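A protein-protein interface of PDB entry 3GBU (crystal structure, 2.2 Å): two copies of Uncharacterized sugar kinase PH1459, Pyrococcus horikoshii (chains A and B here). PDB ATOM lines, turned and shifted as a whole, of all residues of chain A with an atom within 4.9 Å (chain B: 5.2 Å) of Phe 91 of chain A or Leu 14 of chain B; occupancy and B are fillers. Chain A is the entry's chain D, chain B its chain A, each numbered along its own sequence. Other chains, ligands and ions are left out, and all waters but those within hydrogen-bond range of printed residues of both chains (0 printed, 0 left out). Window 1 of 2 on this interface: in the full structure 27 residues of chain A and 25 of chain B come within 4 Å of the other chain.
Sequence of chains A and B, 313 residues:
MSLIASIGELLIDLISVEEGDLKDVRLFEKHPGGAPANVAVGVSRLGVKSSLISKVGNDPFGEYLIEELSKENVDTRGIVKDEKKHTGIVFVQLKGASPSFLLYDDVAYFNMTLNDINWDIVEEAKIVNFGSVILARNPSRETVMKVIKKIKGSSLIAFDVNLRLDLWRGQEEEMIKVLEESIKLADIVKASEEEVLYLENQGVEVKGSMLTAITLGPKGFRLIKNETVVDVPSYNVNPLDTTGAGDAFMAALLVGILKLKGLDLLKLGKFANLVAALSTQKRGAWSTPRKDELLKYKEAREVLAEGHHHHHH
The backbone carbonyl oxygen of Phe 28 of chain B lies within hydrogen-bond range of the backbone NH of Phe 28 of chain A (2.9 Å).
The backbone carbonyl oxygen (O) of Ile 89 of chain A is in hydrogen-bond range of the backbone NH (N) of Tyr 104 of chain A (3.3 Å).
N of Leu 14 of chain B sits at hydrogen-bond distance from O of Val 90 of chain B.
The backbone carbonyl oxygen (O) of Leu 14 of chain A is in hydrogen-bond range of the backbone NH (N) of Val 92 of chain A (2.8 Å).
O of Phe 91 of chain A is in hydrogen-bond range of N of Leu 102 of chain A (2.9 Å).
O of Leu 14 of chain B is in hydrogen-bond range of N of Val 92 of chain B (2.8 Å).
The backbone NH of Leu 14 of chain A lies within hydrogen-bond range of the backbone carbonyl oxygen of Val 90 of chain A (2.9 Å).
Among the printed residues, pairs that only touch across the chains: Ile 89 of chain A with Ile 89 of chain B, Leu 14 of chain A with Phe 91 of chain B, Tyr 104 of chain A with Ile 89 of chain B, Phe 91 of chain A with Leu 14 of chain B, Leu 22 of chain A with Phe 61 of chain B, Phe 91 of chain A with Phe 61 of chain B, Leu 102 of chain A with Phe 61 of chain B, Leu 22 of chain A with Lys 30 of chain B, Ile 89 of chain A with Phe 91 of chain B, Phe 28 of chain A with Phe 61 of chain B, Phe 28 of chain A with Lys 30 of chain B, Phe 91 of chain A with Phe 91 of chain B and Tyr 104 of chain A with Phe 61 of chain B.
Phe 91 of chain A touches just these residues of chain B: Leu 14 (3.4 Å), Phe 61 (3.7 Å) and Phe 91 (3.9 Å).
Leu 14 of chain B touches just one residue of chain A: Phe 91 (3.4 Å).
Printed residues of chain A within 4 Å of Phe 91 of chain B: Leu 14 (3.2 Å), Ile 89 (3.9 Å) and Phe 91 (3.9 Å).
Of the printed residues of chain A, Lys 30 of chain B touches Leu 22 and Phe 28.
Printed residues of chain B within 4 Å of Leu 14 of chain A: Phe 91 (3.2 Å).
Of the printed residues of chain B, Ile 89 of chain A touches Ile 89 and Phe 91.
Of the printed residues of chain A, Phe 61 of chain B touches Leu 22, Phe 28, Phe 91, Leu 102 and Tyr 104.
The nearest residue of chain B that does not touch Phe 91 of chain A is Ile 89 of chain B (4.2 Å).
Of the 13 printed residues of chain B, 6 touch a printed residue of chain A.
Printed residues of chain B that touch a printed residue of chain A: Leu 14, Phe 28, Lys 30, Phe 61, Ile 89 and Phe 91.
Hydrophobic or aromatic side chains of chain B within 4 Å of the printed part of chain A: Leu 14, Phe 61, Ile 89 and Phe 91.
Along chain A the printed residues that touch a printed residue of chain B span positions 14 to 104.
Leu 14 of chain A touches Phe 91 of chain B, and with the chains exchanged Phe 91 of chain A touches Leu 14 of chain B.
Phe 28 of chain B touches its own counterpart, Phe 28 of chain A.
Ile 89 of chain A touches its own counterpart, Ile 89 of chain B.
Ile 89 of chain A touches Phe 91 of chain B, but with the chains exchanged Phe 91 of chain A does not touch Ile 89 of chain B (4.2 Å).
Positions printed for both chains: 14, 28, 89, 90, 91 and 92.
Of the 14 pairs that touch across the chains among the printed residues, 5 have their exchanged pair printed and touching as well.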
ATOM      1  N   LEU A  14      -6.241  17.540 -10.582  1.00  0.00           N
ATOM      2  CA  LEU A  14      -4.788  17.590 -10.567  1.00  0.00           C
ATOM      3  C   LEU A  14      -4.469  16.549  -9.505  1.00  0.00           C
ATOM      4  O   LEU A  14      -4.526  16.807  -8.301  1.00  0.00           O
ATOM      5  CB  LEU A  14      -4.312  18.995 -10.198  1.00  0.00           C
ATOM      6  CG  LEU A  14      -4.760  19.930 -11.334  1.00  0.00           C
ATOM      7  CD1 LEU A  14      -4.868  21.356 -10.847  1.00  0.00           C
ATOM      8  CD2 LEU A  14      -3.810  19.784 -12.518  1.00  0.00           C
ATOM      9  N   LEU A  22      -1.182  17.131   0.604  1.00  0.00           N
ATOM     10  CA  LEU A  22      -1.173  18.056  -0.518  1.00  0.00           C
ATOM     11  C   LEU A  22      -0.097  19.122  -0.336  1.00  0.00           C
ATOM     12  O   LEU A  22       0.485  19.607  -1.310  1.00  0.00           O
ATOM     13  CB  LEU A  22      -2.537  18.726  -0.663  1.00  0.00           C
ATOM     14  CG  LEU A  22      -3.602  17.854  -1.319  1.00  0.00           C
ATOM     15  CD1 LEU A  22      -4.931  18.603  -1.342  1.00  0.00           C
ATOM     16  CD2 LEU A  22      -3.162  17.501  -2.749  1.00  0.00           C
ATOM     17  N   PHE A  28       1.824  16.859  -9.932  1.00  0.00           N
ATOM     18  CA  PHE A  28       0.408  16.625 -10.202  1.00  0.00           C
ATOM     19  C   PHE A  28       0.227  16.264 -11.672  1.00  0.00           C
ATOM     20  O   PHE A  28       0.905  16.806 -12.545  1.00  0.00           O
ATOM     21  CB  PHE A  28      -0.410  17.876  -9.881  1.00  0.00           C
ATOM     22  CG  PHE A  28      -0.377  18.260  -8.434  1.00  0.00           C
ATOM     23  CD1 PHE A  28      -1.253  17.674  -7.527  1.00  0.00           C
ATOM     24  CD2 PHE A  28       0.548  19.185  -7.973  1.00  0.00           C
ATOM     25  CE1 PHE A  28      -1.207  18.003  -6.185  1.00  0.00           C
ATOM     26  CE2 PHE A  28       0.606  19.523  -6.632  1.00  0.00           C
ATOM     27  CZ  PHE A  28      -0.279  18.930  -5.732  1.00  0.00           C
ATOM     28  N   ILE A  89     -11.125  23.407 -11.125  1.00  0.00           N
ATOM     29  CA  ILE A  89      -9.950  22.617 -10.805  1.00  0.00           C
ATOM     30  C   ILE A  89     -10.010  22.146  -9.359  1.00  0.00           C
ATOM     31  O   ILE A  89     -10.551  22.828  -8.480  1.00  0.00           O
ATOM     32  CB  ILE A  89      -8.663  23.438 -10.950  1.00  0.00           C
ATOM     33  CG1 ILE A  89      -8.726  24.630  -9.992  1.00  0.00           C
ATOM     34  CG2 ILE A  89      -8.474  23.876 -12.398  1.00  0.00           C
ATOM     35  CD1 ILE A  89      -7.563  25.577 -10.090  1.00  0.00           C
ATOM     36  N   VAL A  90      -9.432  20.978  -9.122  1.00  0.00           N
ATOM     37  CA  VAL A  90      -9.370  20.421  -7.784  1.00  0.00           C
ATOM     38  C   VAL A  90      -8.101  19.597  -7.686  1.00  0.00           C
ATOM     39  O   VAL A  90      -7.844  18.731  -8.526  1.00  0.00           O
ATOM     40  CB  VAL A  90     -10.597  19.523  -7.473  1.00  0.00           C
ATOM     41  CG1 VAL A  90     -10.811  18.526  -8.593  1.00  0.00           C
ATOM     42  CG2 VAL A  90     -10.387  18.797  -6.156  1.00  0.00           C
ATOM     43  N   PHE A  91      -7.297  19.908  -6.678  1.00  0.00           N
ATOM     44  CA  PHE A  91      -6.057  19.200  -6.404  1.00  0.00           C
ATOM     45  C   PHE A  91      -6.473  18.026  -5.526  1.00  0.00           C
ATOM     46  O   PHE A  91      -7.162  18.208  -4.523  1.00  0.00           O
ATOM     47  CB  PHE A  91      -5.089  20.130  -5.670  1.00  0.00           C
ATOM     48  CG  PHE A  91      -4.630  21.287  -6.504  1.00  0.00           C
ATOM     49  CD1 PHE A  91      -3.498  21.177  -7.314  1.00  0.00           C
ATOM     50  CD2 PHE A  91      -5.354  22.473  -6.521  1.00  0.00           C
ATOM     51  CE1 PHE A  91      -3.098  22.235  -8.127  1.00  0.00           C
ATOM     52  CE2 PHE A  91      -4.962  23.537  -7.333  1.00  0.00           C
ATOM     53  CZ  PHE A  91      -3.834  23.418  -8.136  1.00  0.00           C
ATOM     54  N   VAL A  92      -6.071  16.820  -5.908  1.00  0.00           N
ATOM     55  CA  VAL A  92      -6.472  15.646  -5.148  1.00  0.00           C
ATOM     56  C   VAL A  92      -5.332  14.721  -4.752  1.00  0.00           C
ATOM     57  O   VAL A  92      -4.333  14.590  -5.461  1.00  0.00           O
ATOM     58  CB  VAL A  92      -7.525  14.790  -5.931  1.00  0.00           C
ATOM     59  CG1 VAL A  92      -8.539  15.692  -6.640  1.00  0.00           C
ATOM     60  CG2 VAL A  92      -6.837  13.904  -6.938  1.00  0.00           C
ATOM     61  N   GLN A  93      -5.495  14.100  -3.590  1.00  0.00           N
ATOM     62  CA  GLN A  93      -4.548  13.118  -3.083  1.00  0.00           C
ATOM     63  C   GLN A  93      -5.453  11.929  -2.799  1.00  0.00           C
ATOM     64  O   GLN A  93      -6.190  11.908  -1.808  1.00  0.00           O
ATOM     65  CB  GLN A  93      -3.861  13.599  -1.806  1.00  0.00           C
ATOM     66  CG  GLN A  93      -2.965  12.557  -1.142  1.00  0.00           C
ATOM     67  CD  GLN A  93      -1.963  11.910  -2.100  1.00  0.00           C
ATOM     68  OE1 GLN A  93      -2.316  11.037  -2.909  1.00  0.00           O
ATOM     69  NE2 GLN A  93      -0.704  12.339  -2.011  1.00  0.00           N
ATOM     70  N   SER A 100      -7.423  13.335   0.450  1.00  0.00           N
ATOM     71  CA  SER A 100      -7.886  14.705   0.618  1.00  0.00           C
ATOM     72  C   SER A 100      -7.935  15.472  -0.689  1.00  0.00           C
ATOM     73  O   SER A 100      -7.484  14.986  -1.725  1.00  0.00           O
ATOM     74  CB  SER A 100      -6.970  15.430   1.602  1.00  0.00           C
ATOM     75  OG  SER A 100      -5.620  15.308   1.187  1.00  0.00           O
ATOM     76  N   PHE A 101      -8.478  16.681  -0.629  1.00  0.00           N
ATOM     77  CA  PHE A 101      -8.589  17.519  -1.810  1.00  0.00           C
ATOM     78  C   PHE A 101      -8.673  19.003  -1.462  1.00  0.00           C
ATOM     79  O   PHE A 101      -9.027  19.373  -0.341  1.00  0.00           O
ATOM     80  CB  PHE A 101      -9.820  17.096  -2.630  1.00  0.00           C
ATOM     81  CG  PHE A 101     -11.136  17.415  -1.970  1.00  0.00           C
ATOM     82  CD1 PHE A 101     -11.797  18.611  -2.242  1.00  0.00           C
ATOM     83  CD2 PHE A 101     -11.707  16.527  -1.058  1.00  0.00           C
ATOM     84  CE1 PHE A 101     -13.012  18.923  -1.614  1.00  0.00           C
ATOM     85  CE2 PHE A 101     -12.920  16.828  -0.424  1.00  0.00           C
ATOM     86  CZ  PHE A 101     -13.574  18.031  -0.703  1.00  0.00           C
ATOM     87  N   LEU A 102      -8.313  19.837  -2.431  1.00  0.00           N
ATOM     88  CA  LEU A 102      -8.367  21.289  -2.294  1.00  0.00           C
ATOM     89  C   LEU A 102      -9.071  21.767  -3.545  1.00  0.00           C
ATOM     90  O   LEU A 102      -8.465  21.836  -4.621  1.00  0.00           O
ATOM     91  CB  LEU A 102      -6.967  21.907  -2.233  1.00  0.00           C
ATOM     92  CG  LEU A 102      -6.950  23.441  -2.163  1.00  0.00           C
ATOM     93  CD1 LEU A 102      -7.808  23.934  -0.993  1.00  0.00           C
ATOM     94  CD2 LEU A 102      -5.510  23.918  -2.019  1.00  0.00           C
ATOM     95  N   TYR A 104     -11.158  24.585  -5.786  1.00  0.00           N
ATOM     96  CA  TYR A 104     -11.301  26.023  -5.978  1.00  0.00           C
ATOM     97  C   TYR A 104     -12.734  26.273  -6.440  1.00  0.00           C
ATOM     98  O   TYR A 104     -13.150  25.794  -7.488  1.00  0.00           O
ATOM     99  CB  TYR A 104     -10.255  26.519  -6.990  1.00  0.00           C
ATOM    100  CG  TYR A 104      -8.887  26.641  -6.356  1.00  0.00           C
ATOM    101  CD1 TYR A 104      -8.197  25.509  -5.920  1.00  0.00           C
ATOM    102  CD2 TYR A 104      -8.331  27.895  -6.085  1.00  0.00           C
ATOM    103  CE1 TYR A 104      -6.992  25.618  -5.218  1.00  0.00           C
ATOM    104  CE2 TYR A 104      -7.131  28.015  -5.383  1.00  0.00           C
ATOM    105  CZ  TYR A 104      -6.470  26.873  -4.949  1.00  0.00           C
ATOM    106  OH  TYR A 104      -5.320  26.994  -4.204  1.00  0.00           O
ATOM    107  N   ILE B  12       1.139  29.656  -5.630  1.00  0.00           N
ATOM    108  CA  ILE B  12       1.696  28.383  -6.063  1.00  0.00           C
ATOM    109  C   ILE B  12       1.829  28.405  -7.583  1.00  0.00           C
ATOM    110  O   ILE B  12       0.842  28.642  -8.286  1.00  0.00           O
ATOM    111  CB  ILE B  12       0.754  27.196  -5.748  1.00  0.00           C
ATOM    112  CG1 ILE B  12       0.533  27.047  -4.244  1.00  0.00           C
ATOM    113  CG2 ILE B  12       1.350  25.907  -6.343  1.00  0.00           C
ATOM    114  CD1 ILE B  12       1.712  26.445  -3.501  1.00  0.00           C
ATOM    115  N   ASP B  13       3.041  28.187  -8.080  1.00  0.00           N
ATOM    116  CA  ASP B  13       3.266  28.104  -9.517  1.00  0.00           C
ATOM    117  C   ASP B  13       3.175  26.611  -9.862  1.00  0.00           C
ATOM    118  O   ASP B  13       3.869  25.791  -9.263  1.00  0.00           O
ATOM    119  CB  ASP B  13       4.674  28.583  -9.916  1.00  0.00           C
ATOM    120  CG  ASP B  13       4.806  30.093  -9.971  1.00  0.00           C
ATOM    121  OD1 ASP B  13       3.789  30.787 -10.102  1.00  0.00           O
ATOM    122  OD2 ASP B  13       5.947  30.591  -9.904  1.00  0.00           O
ATOM    123  N   LEU B  14       2.307  26.261 -10.802  1.00  0.00           N
ATOM    124  CA  LEU B  14       2.185  24.876 -11.247  1.00  0.00           C
ATOM    125  C   LEU B  14       2.886  24.928 -12.602  1.00  0.00           C
ATOM    126  O   LEU B  14       2.325  25.352 -13.615  1.00  0.00           O
ATOM    127  CB  LEU B  14       0.709  24.491 -11.361  1.00  0.00           C
ATOM    128  CG  LEU B  14       0.123  24.530  -9.937  1.00  0.00           C
ATOM    129  CD1 LEU B  14      -1.367  24.780  -9.959  1.00  0.00           C
ATOM    130  CD2 LEU B  14       0.461  23.241  -9.227  1.00  0.00           C
ATOM    131  N   ILE B  15       4.149  24.526 -12.578  1.00  0.00           N
ATOM    132  CA  ILE B  15       5.015  24.576 -13.743  1.00  0.00           C
ATOM    133  C   ILE B  15       4.969  23.339 -14.623  1.00  0.00           C
ATOM    134  O   ILE B  15       5.251  22.232 -14.166  1.00  0.00           O
ATOM    135  CB  ILE B  15       6.468  24.847 -13.276  1.00  0.00           C
ATOM    136  CG1 ILE B  15       6.486  26.132 -12.431  1.00  0.00           C
ATOM    137  CG2 ILE B  15       7.404  24.958 -14.474  1.00  0.00           C
ATOM    138  CD1 ILE B  15       7.839  26.509 -11.858  1.00  0.00           C
ATOM    139  N   SER B  16       4.596  23.535 -15.884  1.00  0.00           N
ATOM    140  CA  SER B  16       4.536  22.441 -16.854  1.00  0.00           C
ATOM    141  C   SER B  16       5.910  21.775 -16.907  1.00  0.00           C
ATOM    142  O   SER B  16       6.910  22.452 -17.140  1.00  0.00           O
ATOM    143  CB  SER B  16       4.199  22.989 -18.241  1.00  0.00           C
ATOM    144  OG  SER B  16       2.910  23.573 -18.267  1.00  0.00           O
ATOM    145  N   PHE B  28       2.603  18.733 -13.856  1.00  0.00           N
ATOM    146  CA  PHE B  28       2.890  20.034 -13.291  1.00  0.00           C
ATOM    147  C   PHE B  28       3.633  19.836 -11.978  1.00  0.00           C
ATOM    148  O   PHE B  28       3.284  18.970 -11.175  1.00  0.00           O
ATOM    149  CB  PHE B  28       1.589  20.793 -13.037  1.00  0.00           C
ATOM    150  CG  PHE B  28       0.838  21.147 -14.292  1.00  0.00           C
ATOM    151  CD1 PHE B  28       1.069  22.359 -14.939  1.00  0.00           C
ATOM    152  CD2 PHE B  28      -0.097  20.272 -14.826  1.00  0.00           C
ATOM    153  CE1 PHE B  28       0.374  22.692 -16.103  1.00  0.00           C
ATOM    154  CE2 PHE B  28      -0.795  20.596 -15.988  1.00  0.00           C
ATOM    155  CZ  PHE B  28      -0.557  21.810 -16.625  1.00  0.00           C
ATOM    156  N   GLU B  29       4.660  20.649 -11.780  1.00  0.00           N
ATOM    157  CA  GLU B  29       5.487  20.606 -10.587  1.00  0.00           C
ATOM    158  C   GLU B  29       5.167  21.884  -9.801  1.00  0.00           C
ATOM    159  O   GLU B  29       5.220  22.992 -10.348  1.00  0.00           O
ATOM    160  CB  GLU B  29       6.961  20.565 -11.015  1.00  0.00           C
ATOM    161  CG  GLU B  29       7.955  20.336  -9.904  1.00  0.00           C
ATOM    162  CD  GLU B  29       9.403  20.255 -10.413  1.00  0.00           C
ATOM    163  OE1 GLU B  29       9.882  21.234 -11.052  1.00  0.00           O
ATOM    164  OE2 GLU B  29      10.054  19.207 -10.165  1.00  0.00           O
ATOM    165  N   LYS B  30       4.826  21.744  -8.526  1.00  0.00           N
ATOM    166  CA  LYS B  30       4.477  22.923  -7.738  1.00  0.00           C
ATOM    167  C   LYS B  30       5.671  23.550  -7.022  1.00  0.00           C
ATOM    168  O   LYS B  30       6.508  22.850  -6.452  1.00  0.00           O
ATOM    169  CB  LYS B  30       3.349  22.587  -6.743  1.00  0.00           C
ATOM    170  CG  LYS B  30       3.767  22.213  -5.333  1.00  0.00           C
ATOM    171  CD  LYS B  30       2.516  22.113  -4.434  1.00  0.00           C
ATOM    172  CE  LYS B  30       2.849  22.227  -2.953  1.00  0.00           C
ATOM    173  NZ  LYS B  30       3.796  21.176  -2.508  1.00  0.00           N
ATOM    174  N   PHE B  61      -1.758  24.450   0.627  1.00  0.00           N
ATOM    175  CA  PHE B  61      -0.878  25.265  -0.210  1.00  0.00           C
ATOM    176  C   PHE B  61      -0.424  26.525   0.498  1.00  0.00           C
ATOM    177  O   PHE B  61       0.692  26.999   0.287  1.00  0.00           O
ATOM    178  CB  PHE B  61      -1.569  25.591  -1.539  1.00  0.00           C
ATOM    179  CG  PHE B  61      -1.613  24.422  -2.498  1.00  0.00           C
ATOM    180  CD1 PHE B  61      -1.001  23.212  -2.165  1.00  0.00           C
ATOM    181  CD2 PHE B  61      -2.252  24.529  -3.734  1.00  0.00           C
ATOM    182  CE1 PHE B  61      -1.026  22.131  -3.046  1.00  0.00           C
ATOM    183  CE2 PHE B  61      -2.280  23.452  -4.616  1.00  0.00           C
ATOM    184  CZ  PHE B  61      -1.664  22.250  -4.266  1.00  0.00           C
ATOM    185  N   ILE B  89      -2.917  30.552  -7.118  1.00  0.00           N
ATOM    186  CA  ILE B  89      -2.326  29.537  -7.992  1.00  0.00           C
ATOM    187  C   ILE B  89      -2.221  30.025  -9.439  1.00  0.00           C
ATOM    188  O   ILE B  89      -3.046  30.813  -9.899  1.00  0.00           O
ATOM    189  CB  ILE B  89      -3.186  28.254  -8.034  1.00  0.00           C
ATOM    190  CG1 ILE B  89      -4.615  28.618  -8.445  1.00  0.00           C
ATOM    191  CG2 ILE B  89      -3.174  27.549  -6.669  1.00  0.00           C
ATOM    192  CD1 ILE B  89      -5.503  27.435  -8.692  1.00  0.00           C
ATOM    193  N   VAL B  90      -1.197  29.560 -10.148  1.00  0.00           N
ATOM    194  CA  VAL B  90      -1.039  29.891 -11.549  1.00  0.00           C
ATOM    195  C   VAL B  90      -0.398  28.715 -12.251  1.00  0.00           C
ATOM    196  O   VAL B  90       0.613  28.181 -11.797  1.00  0.00           O
ATOM    197  CB  VAL B  90      -0.155  31.146 -11.796  1.00  0.00           C
ATOM    198  CG1 VAL B  90       1.238  30.925 -11.235  1.00  0.00           C
ATOM    199  CG2 VAL B  90      -0.081  31.448 -13.309  1.00  0.00           C
ATOM    200  N   PHE B  91      -1.018  28.297 -13.342  1.00  0.00           N
ATOM    201  CA  PHE B  91      -0.504  27.210 -14.149  1.00  0.00           C
ATOM    202  C   PHE B  91       0.377  27.913 -15.181  1.00  0.00           C
ATOM    203  O   PHE B  91      -0.062  28.860 -15.829  1.00  0.00           O
ATOM    204  CB  PHE B  91      -1.665  26.477 -14.816  1.00  0.00           C
ATOM    205  CG  PHE B  91      -2.518  25.701 -13.852  1.00  0.00           C
ATOM    206  CD1 PHE B  91      -2.178  24.397 -13.500  1.00  0.00           C
ATOM    207  CD2 PHE B  91      -3.630  26.292 -13.249  1.00  0.00           C
ATOM    208  CE1 PHE B  91      -2.930  23.687 -12.553  1.00  0.00           C
ATOM    209  CE2 PHE B  91      -4.386  25.592 -12.302  1.00  0.00           C
ATOM    210  CZ  PHE B  91      -4.032  24.288 -11.954  1.00  0.00           C
ATOM    211  N   VAL B  92       1.621  27.474 -15.320  1.00  0.00           N
ATOM    212  CA  VAL B  92       2.509  28.119 -16.262  1.00  0.00           C
ATOM    213  C   VAL B  92       3.285  27.198 -17.187  1.00  0.00           C
ATOM    214  O   VAL B  92       3.675  26.084 -16.828  1.00  0.00           O
ATOM    215  CB  VAL B  92       3.549  29.029 -15.545  1.00  0.00           C
ATOM    216  CG1 VAL B  92       2.886  29.840 -14.441  1.00  0.00           C
ATOM    217  CG2 VAL B  92       4.666  28.199 -14.978  1.00  0.00           C
